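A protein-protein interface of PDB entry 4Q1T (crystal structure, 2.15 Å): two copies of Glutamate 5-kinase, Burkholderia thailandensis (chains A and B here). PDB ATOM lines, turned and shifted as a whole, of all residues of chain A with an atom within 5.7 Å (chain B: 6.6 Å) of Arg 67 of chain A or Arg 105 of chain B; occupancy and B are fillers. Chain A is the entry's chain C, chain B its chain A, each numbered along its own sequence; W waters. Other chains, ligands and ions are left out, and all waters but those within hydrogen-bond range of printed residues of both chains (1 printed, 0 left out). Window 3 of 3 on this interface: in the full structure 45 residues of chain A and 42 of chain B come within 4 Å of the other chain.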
ATOM      1  N   ALA A  62      21.831 -14.527  23.117  1.00  0.00           N
ATOM      2  CA  ALA A  62      21.072 -13.899  24.182  1.00  0.00           C
ATOM      3  C   ALA A  62      20.776 -14.854  25.319  1.00  0.00           C
ATOM      4  O   ALA A  62      20.861 -14.464  26.474  1.00  0.00           O
ATOM      5  CB  ALA A  62      19.748 -13.340  23.652  1.00  0.00           C
ATOM      6  N   GLU A  63      20.409 -16.091  25.009  1.00  0.00           N
ATOM      7  CA  GLU A  63      20.137 -17.099  26.039  1.00  0.00           C
ATOM      8  C   GLU A  63      21.414 -17.465  26.758  1.00  0.00           C
ATOM      9  O   GLU A  63      21.439 -17.611  27.980  1.00  0.00           O
ATOM     10  CB  GLU A  63      19.508 -18.336  25.405  1.00  0.00           C
ATOM     11  CG  GLU A  63      19.178 -19.493  26.333  1.00  0.00           C
ATOM     12  CD  GLU A  63      18.220 -19.144  27.466  1.00  0.00           C
ATOM     13  OE1 GLU A  63      17.618 -18.070  27.464  1.00  0.00           O
ATOM     14  OE2 GLU A  63      18.079 -19.959  28.399  1.00  0.00           O
ATOM     15  N   GLY A  64      22.490 -17.614  25.991  1.00  0.00           N
ATOM     16  CA  GLY A  64      23.773 -17.926  26.566  1.00  0.00           C
ATOM     17  C   GLY A  64      24.220 -16.849  27.537  1.00  0.00           C
ATOM     18  O   GLY A  64      24.705 -17.155  28.617  1.00  0.00           O
ATOM     19  N   MET A  65      24.070 -15.601  27.121  1.00  0.00           N
ATOM     20  CA  MET A  65      24.415 -14.457  27.950  1.00  0.00           C
ATOM     21  C   MET A  65      23.673 -14.555  29.270  1.00  0.00           C
ATOM     22  O   MET A  65      24.287 -14.466  30.323  1.00  0.00           O
ATOM     23  CB  MET A  65      24.062 -13.135  27.263  1.00  0.00           C
ATOM     24  CG  MET A  65      25.076 -12.646  26.250  1.00  0.00           C
ATOM     25  SD  MET A  65      24.337 -11.403  25.152  1.00  0.00           S
ATOM     26  CE  MET A  65      24.046 -10.088  26.372  1.00  0.00           C
ATOM     27  N   GLN A  66      22.364 -14.776  29.206  1.00  0.00           N
ATOM     28  CA  GLN A  66      21.559 -14.882  30.414  1.00  0.00           C
ATOM     29  C   GLN A  66      22.049 -16.005  31.323  1.00  0.00           C
ATOM     30  O   GLN A  66      22.209 -15.815  32.540  1.00  0.00           O
ATOM     31  CB  GLN A  66      20.087 -15.124  30.063  1.00  0.00           C
ATOM     32  N   ARG A  67      22.313 -17.160  30.736  1.00  0.00           N
ATOM     33  CA  ARG A  67      22.759 -18.310  31.521  1.00  0.00           C
ATOM     34  C   ARG A  67      24.158 -18.130  32.113  1.00  0.00           C
ATOM     35  O   ARG A  67      24.465 -18.725  33.142  1.00  0.00           O
ATOM     36  CB  ARG A  67      22.708 -19.579  30.674  1.00  0.00           C
ATOM     37  CG  ARG A  67      21.302 -20.119  30.523  1.00  0.00           C
ATOM     38  CD  ARG A  67      21.231 -21.168  29.424  1.00  0.00           C
ATOM     39  NE  ARG A  67      19.863 -21.677  29.317  1.00  0.00           N
ATOM     40  CZ  ARG A  67      19.498 -22.954  29.438  1.00  0.00           C
ATOM     41  NH1 ARG A  67      20.394 -23.925  29.612  1.00  0.00           N
ATOM     42  NH2 ARG A  67      18.214 -23.265  29.358  1.00  0.00           N
ATOM     43  N   LEU A  68      24.996 -17.320  31.468  1.00  0.00           N
ATOM     44  CA  LEU A  68      26.338 -17.064  31.973  1.00  0.00           C
ATOM     45  C   LEU A  68      26.437 -15.827  32.855  1.00  0.00           C
ATOM     46  O   LEU A  68      27.514 -15.511  33.355  1.00  0.00           O
ATOM     47  CB  LEU A  68      27.309 -16.937  30.804  1.00  0.00           C
ATOM     48  CG  LEU A  68      27.526 -18.224  30.004  1.00  0.00           C
ATOM     49  CD1 LEU A  68      28.233 -17.904  28.689  1.00  0.00           C
ATOM     50  CD2 LEU A  68      28.311 -19.228  30.835  1.00  0.00           C
ATOM     51  N   GLY A  69      25.325 -15.124  33.049  1.00  0.00           N
ATOM     52  CA  GLY A  69      25.306 -13.949  33.898  1.00  0.00           C
ATOM     53  C   GLY A  69      25.885 -12.699  33.259  1.00  0.00           C
ATOM     54  O   GLY A  69      26.370 -11.809  33.969  1.00  0.00           O
ATOM     55  N   VAL A  86      26.256 -22.312  24.858  1.00  0.00           N
ATOM     56  CA  VAL A  86      25.467 -22.418  26.069  1.00  0.00           C
ATOM     57  C   VAL A  86      23.999 -22.168  25.702  1.00  0.00           C
ATOM     58  O   VAL A  86      23.126 -22.891  26.138  1.00  0.00           O
ATOM     59  CB  VAL A  86      25.943 -21.424  27.140  1.00  0.00           C
ATOM     60  CG1 VAL A  86      24.978 -21.361  28.311  1.00  0.00           C
ATOM     61  CG2 VAL A  86      27.332 -21.818  27.634  1.00  0.00           C
ATOM     62  N   GLY A  87      23.764 -21.136  24.899  1.00  0.00           N
ATOM     63  CA  GLY A  87      22.412 -20.705  24.609  1.00  0.00           C
ATOM     64  C   GLY A  87      21.625 -21.646  23.705  1.00  0.00           C
ATOM     65  O   GLY A  87      20.425 -21.752  23.838  1.00  0.00           O
ATOM     66  N   MET A  89      21.519 -24.834  23.736  1.00  0.00           N
ATOM     67  CA  MET A  89      20.862 -25.823  24.590  1.00  0.00           C
ATOM     68  C   MET A  89      19.527 -25.352  25.148  1.00  0.00           C
ATOM     69  O   MET A  89      18.547 -26.104  25.159  1.00  0.00           O
ATOM     70  CB  MET A  89      21.791 -26.095  25.779  1.00  0.00           C
ATOM     71  CG  MET A  89      21.421 -27.270  26.713  1.00  0.00           C
ATOM     72  SD  MET A  89      22.124 -28.715  25.931  1.00  0.00           S
ATOM     73  CE  MET A  89      22.971 -29.520  27.279  1.00  0.00           C
ATOM     74  N   GLY A  90      19.496 -24.111  25.627  1.00  0.00           N
ATOM     75  CA  GLY A  90      18.284 -23.534  26.183  1.00  0.00           C
ATOM     76  C   GLY A  90      17.251 -23.249  25.113  1.00  0.00           C
ATOM     77  O   GLY A  90      16.084 -23.547  25.285  1.00  0.00           O
ATOM     78  N   LEU A  91      17.690 -22.670  24.007  1.00  0.00           N
ATOM     79  CA  LEU A  91      16.787 -22.254  22.941  1.00  0.00           C
ATOM     80  C   LEU A  91      15.990 -23.455  22.427  1.00  0.00           C
ATOM     81  O   LEU A  91      14.782 -23.360  22.210  1.00  0.00           O
ATOM     82  CB  LEU A  91      17.570 -21.583  21.815  1.00  0.00           C
ATOM     83  CG  LEU A  91      16.767 -21.060  20.621  1.00  0.00           C
ATOM     84  CD1 LEU A  91      15.738 -20.011  21.032  1.00  0.00           C
ATOM     85  CD2 LEU A  91      17.727 -20.488  19.584  1.00  0.00           C
ATOM     86  N   GLN A  93      15.588 -26.494  24.020  1.00  0.00           N
ATOM     87  CA  GLN A  93      14.765 -27.076  25.104  1.00  0.00           C
ATOM     88  C   GLN A  93      13.423 -26.364  25.253  1.00  0.00           C
ATOM     89  O   GLN A  93      12.415 -27.010  25.512  1.00  0.00           O
ATOM     90  CB  GLN A  93      15.505 -27.081  26.446  1.00  0.00           C
ATOM     91  N   GLU B  96      21.191 -31.574  30.802  1.00  0.00           N
ATOM     92  CA  GLU B  96      21.071 -30.203  31.277  1.00  0.00           C
ATOM     93  C   GLU B  96      20.303 -30.162  32.611  1.00  0.00           C
ATOM     94  O   GLU B  96      20.767 -29.543  33.572  1.00  0.00           O
ATOM     95  CB  GLU B  96      20.379 -29.307  30.250  1.00  0.00           C
ATOM     96  N   PHE B  99      22.403 -31.817  35.459  1.00  0.00           N
ATOM     97  CA  PHE B  99      23.505 -30.916  35.802  1.00  0.00           C
ATOM     98  C   PHE B  99      23.032 -29.626  36.485  1.00  0.00           C
ATOM     99  O   PHE B  99      23.690 -29.142  37.405  1.00  0.00           O
ATOM    100  CB  PHE B  99      24.367 -30.559  34.586  1.00  0.00           C
ATOM    101  CG  PHE B  99      25.401 -31.601  34.251  1.00  0.00           C
ATOM    102  CD1 PHE B  99      26.414 -31.910  35.148  1.00  0.00           C
ATOM    103  CD2 PHE B  99      25.363 -32.273  33.039  1.00  0.00           C
ATOM    104  CE1 PHE B  99      27.351 -32.887  34.852  1.00  0.00           C
ATOM    105  CE2 PHE B  99      26.308 -33.241  32.738  1.00  0.00           C
ATOM    106  CZ  PHE B  99      27.299 -33.549  33.641  1.00  0.00           C
ATOM    107  N   ALA B 100      21.905 -29.088  36.029  1.00  0.00           N
ATOM    108  CA  ALA B 100      21.279 -27.914  36.653  1.00  0.00           C
ATOM    109  C   ALA B 100      20.994 -28.102  38.138  1.00  0.00           C
ATOM    110  O   ALA B 100      21.126 -27.163  38.914  1.00  0.00           O
ATOM    111  CB  ALA B 100      19.994 -27.547  35.935  1.00  0.00           C
ATOM    112  N   GLY B 103      23.871 -27.000  39.976  1.00  0.00           N
ATOM    113  CA  GLY B 103      24.352 -25.658  39.630  1.00  0.00           C
ATOM    114  C   GLY B 103      25.347 -25.588  38.485  1.00  0.00           C
ATOM    115  O   GLY B 103      26.099 -24.610  38.362  1.00  0.00           O
ATOM    116  N   ILE B 104      25.357 -26.607  37.629  1.00  0.00           N
ATOM    117  CA  ILE B 104      26.303 -26.645  36.521  1.00  0.00           C
ATOM    118  C   ILE B 104      25.624 -26.349  35.181  1.00  0.00           C
ATOM    119  O   ILE B 104      24.616 -26.956  34.841  1.00  0.00           O
ATOM    120  CB  ILE B 104      27.052 -27.999  36.475  1.00  0.00           C
ATOM    121  CG1 ILE B 104      27.962 -28.115  37.713  1.00  0.00           C
ATOM    122  CG2 ILE B 104      27.915 -28.113  35.226  1.00  0.00           C
ATOM    123  CD1 ILE B 104      28.270 -29.534  38.139  1.00  0.00           C
ATOM    124  N   ARG B 105      26.202 -25.398  34.452  1.00  0.00           N
ATOM    125  CA  ARG B 105      25.813 -25.101  33.073  1.00  0.00           C
ATOM    126  C   ARG B 105      26.438 -26.090  32.107  1.00  0.00           C
ATOM    127  O   ARG B 105      27.571 -26.538  32.311  1.00  0.00           O
ATOM    128  CB  ARG B 105      26.285 -23.709  32.653  1.00  0.00           C
ATOM    129  CG  ARG B 105      25.341 -22.602  33.042  1.00  0.00           C
ATOM    130  CD  ARG B 105      25.646 -21.997  34.379  1.00  0.00           C
ATOM    131  NE  ARG B 105      24.537 -21.154  34.759  1.00  0.00           N
ATOM    132  CZ  ARG B 105      24.411 -20.605  35.950  1.00  0.00           C
ATOM    133  NH1 ARG B 105      25.348 -20.813  36.864  1.00  0.00           N
ATOM    134  NH2 ARG B 105      23.349 -19.860  36.212  1.00  0.00           N
ATOM    135  N   THR B 106      25.693 -26.404  31.056  1.00  0.00           N
ATOM    136  CA  THR B 106      26.163 -27.266  30.004  1.00  0.00           C
ATOM    137  C   THR B 106      26.052 -26.528  28.672  1.00  0.00           C
ATOM    138  O   THR B 106      25.383 -25.517  28.557  1.00  0.00           O
ATOM    139  CB  THR B 106      25.343 -28.553  29.918  1.00  0.00           C
ATOM    140  OG1 THR B 106      23.966 -28.215  29.714  1.00  0.00           O
ATOM    141  CG2 THR B 106      25.459 -29.357  31.196  1.00  0.00           C
ATOM    142  N   ALA B 107      26.737 -27.048  27.675  1.00  0.00           N
ATOM    143  CA  ALA B 107      26.644 -26.513  26.347  1.00  0.00           C
ATOM    144  C   ALA B 107      26.636 -27.683  25.372  1.00  0.00           C
ATOM    145  O   ALA B 107      27.249 -28.715  25.645  1.00  0.00           O
ATOM    146  CB  ALA B 107      27.846 -25.611  26.083  1.00  0.00           C
ATOM    147  N   LEU B 135      35.148 -20.913  31.840  1.00  0.00           N
ATOM    148  CA  LEU B 135      33.912 -20.402  32.459  1.00  0.00           C
ATOM    149  C   LEU B 135      33.180 -21.435  33.322  1.00  0.00           C
ATOM    150  O   LEU B 135      32.140 -21.140  33.915  1.00  0.00           O
ATOM    151  CB  LEU B 135      32.940 -19.887  31.387  1.00  0.00           C
ATOM    152  CG  LEU B 135      33.445 -18.723  30.536  1.00  0.00           C
ATOM    153  CD1 LEU B 135      32.604 -18.541  29.281  1.00  0.00           C
ATOM    154  CD2 LEU B 135      33.460 -17.436  31.363  1.00  0.00           C
ATOM    155  N   GLY B 136      33.721 -22.641  33.416  1.00  0.00           N
ATOM    156  CA  GLY B 136      33.165 -23.646  34.329  1.00  0.00           C
ATOM    157  C   GLY B 136      31.967 -24.350  33.748  1.00  0.00           C
ATOM    158  O   GLY B 136      31.219 -24.950  34.484  1.00  0.00           O
ATOM    159  N   VAL B 137      31.792 -24.277  32.429  1.00  0.00           N
ATOM    160  CA  VAL B 137      30.714 -24.965  31.748  1.00  0.00           C
ATOM    161  C   VAL B 137      31.169 -26.382  31.401  1.00  0.00           C
ATOM    162  O   VAL B 137      32.345 -26.597  31.116  1.00  0.00           O
ATOM    163  CB  VAL B 137      30.307 -24.206  30.461  1.00  0.00           C
ATOM    164  CG1 VAL B 137      29.250 -24.968  29.668  1.00  0.00           C
ATOM    165  CG2 VAL B 137      29.798 -22.806  30.810  1.00  0.00           C
ATOM    166  N   VAL B 138      30.249 -27.351  31.431  1.00  0.00           N
ATOM    167  CA  VAL B 138      30.543 -28.711  30.951  1.00  0.00           C
ATOM    168  C   VAL B 138      30.069 -28.860  29.497  1.00  0.00           C
ATOM    169  O   VAL B 138      28.872 -28.892  29.259  1.00  0.00           O
ATOM    170  CB  VAL B 138      29.844 -29.764  31.801  1.00  0.00           C
ATOM    171  CG1 VAL B 138      30.040 -31.144  31.197  1.00  0.00           C
ATOM    172  CG2 VAL B 138      30.378 -29.738  33.247  1.00  0.00           C
ATOM    173  N   PRO B 139      31.003 -28.885  28.529  1.00  0.00           N
ATOM    174  CA  PRO B 139      30.601 -29.106  27.166  1.00  0.00           C
ATOM    175  C   PRO B 139      30.173 -30.530  26.947  1.00  0.00           C
ATOM    176  O   PRO B 139      30.764 -31.457  27.514  1.00  0.00           O
ATOM    177  CB  PRO B 139      31.870 -28.826  26.369  1.00  0.00           C
ATOM    178  CG  PRO B 139      32.757 -28.044  27.275  1.00  0.00           C
ATOM    179  CD  PRO B 139      32.430 -28.538  28.634  1.00  0.00           C
HETATM  180  O   HOH W   1      22.819 -24.015  28.359  1.00  0.00           O
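O of Arg 67 of chain A sits at hydrogen-bond distance from NE of Arg 105 of chain B.
N of Ala 107 of chain B is in hydrogen-bond range of O of Val 138 of chain B, at 3.2 Å.
OE2 of Glu 63 of chain A lies within salt-bridge range of NE of Arg 67 of chain A (2.6 Å).
The backbone NH (N) of Val 138 of chain B is in hydrogen-bond range of the backbone carbonyl oxygen (O) of Arg 105 of chain B, at 2.9 Å.
Among the printed residues, merely in contact across the chains: Leu 68 of chain A with Val 137 of chain B (3.9 Å), Val 86 of chain A with Thr 106 of chain B (3.98 Å), Val 86 of chain A with Ala 107 of chain B (3.9 Å), Met 89 of chain A with Glu 96 of chain B (3.9 Å) and Met 89 of chain A with Thr 106 of chain B (2.9 Å).
Glu 63 of chain A touches none of the printed residues of chain B.
Of the printed residues of chain B, Leu 68 of chain A touches Val 137.
Leu 91 of chain A touches none of the printed residues of chain B.
Printed residues of chain A within 4 Å of Glu 96 of chain B: Met 89 (3.9 Å).
Of the printed residues of chain A, Thr 106 of chain B touches Val 86 (3.98 Å) and Met 89 (2.9 Å).
Printed residues of chain A within 4 Å of Ala 107 of chain B: Val 86 (3.9 Å).
Printed residues of chain A within 4 Å of Val 137 of chain B: Leu 68.
Hydrophobic or aromatic side chains of chain A that line the printed part of chain B: Leu 68 and Met 89.
Of the 13 printed residues of chain B, 5 touch a printed residue of chain A.
Hydrophobic or aromatic side chains of chain B that line the printed part of chain A: Ala 107 and Val 137.
Among the printed residues, no Asp or Glu carboxylate lies within 4 Å of a Lys or Arg side-chain nitrogen of the other chain.
No position is printed for both chains.
Of the 6 pairs that touch across the chains among the printed residues, none has its exchanged pair printed and touching as well.
Water W1 lies within hydrogen-bond range of O of Val 86 of chain A (2.5 Å), NH1 of Arg 67 of chain A (2.7 Å) and O of Thr 106 of chain B (3.0 Å).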
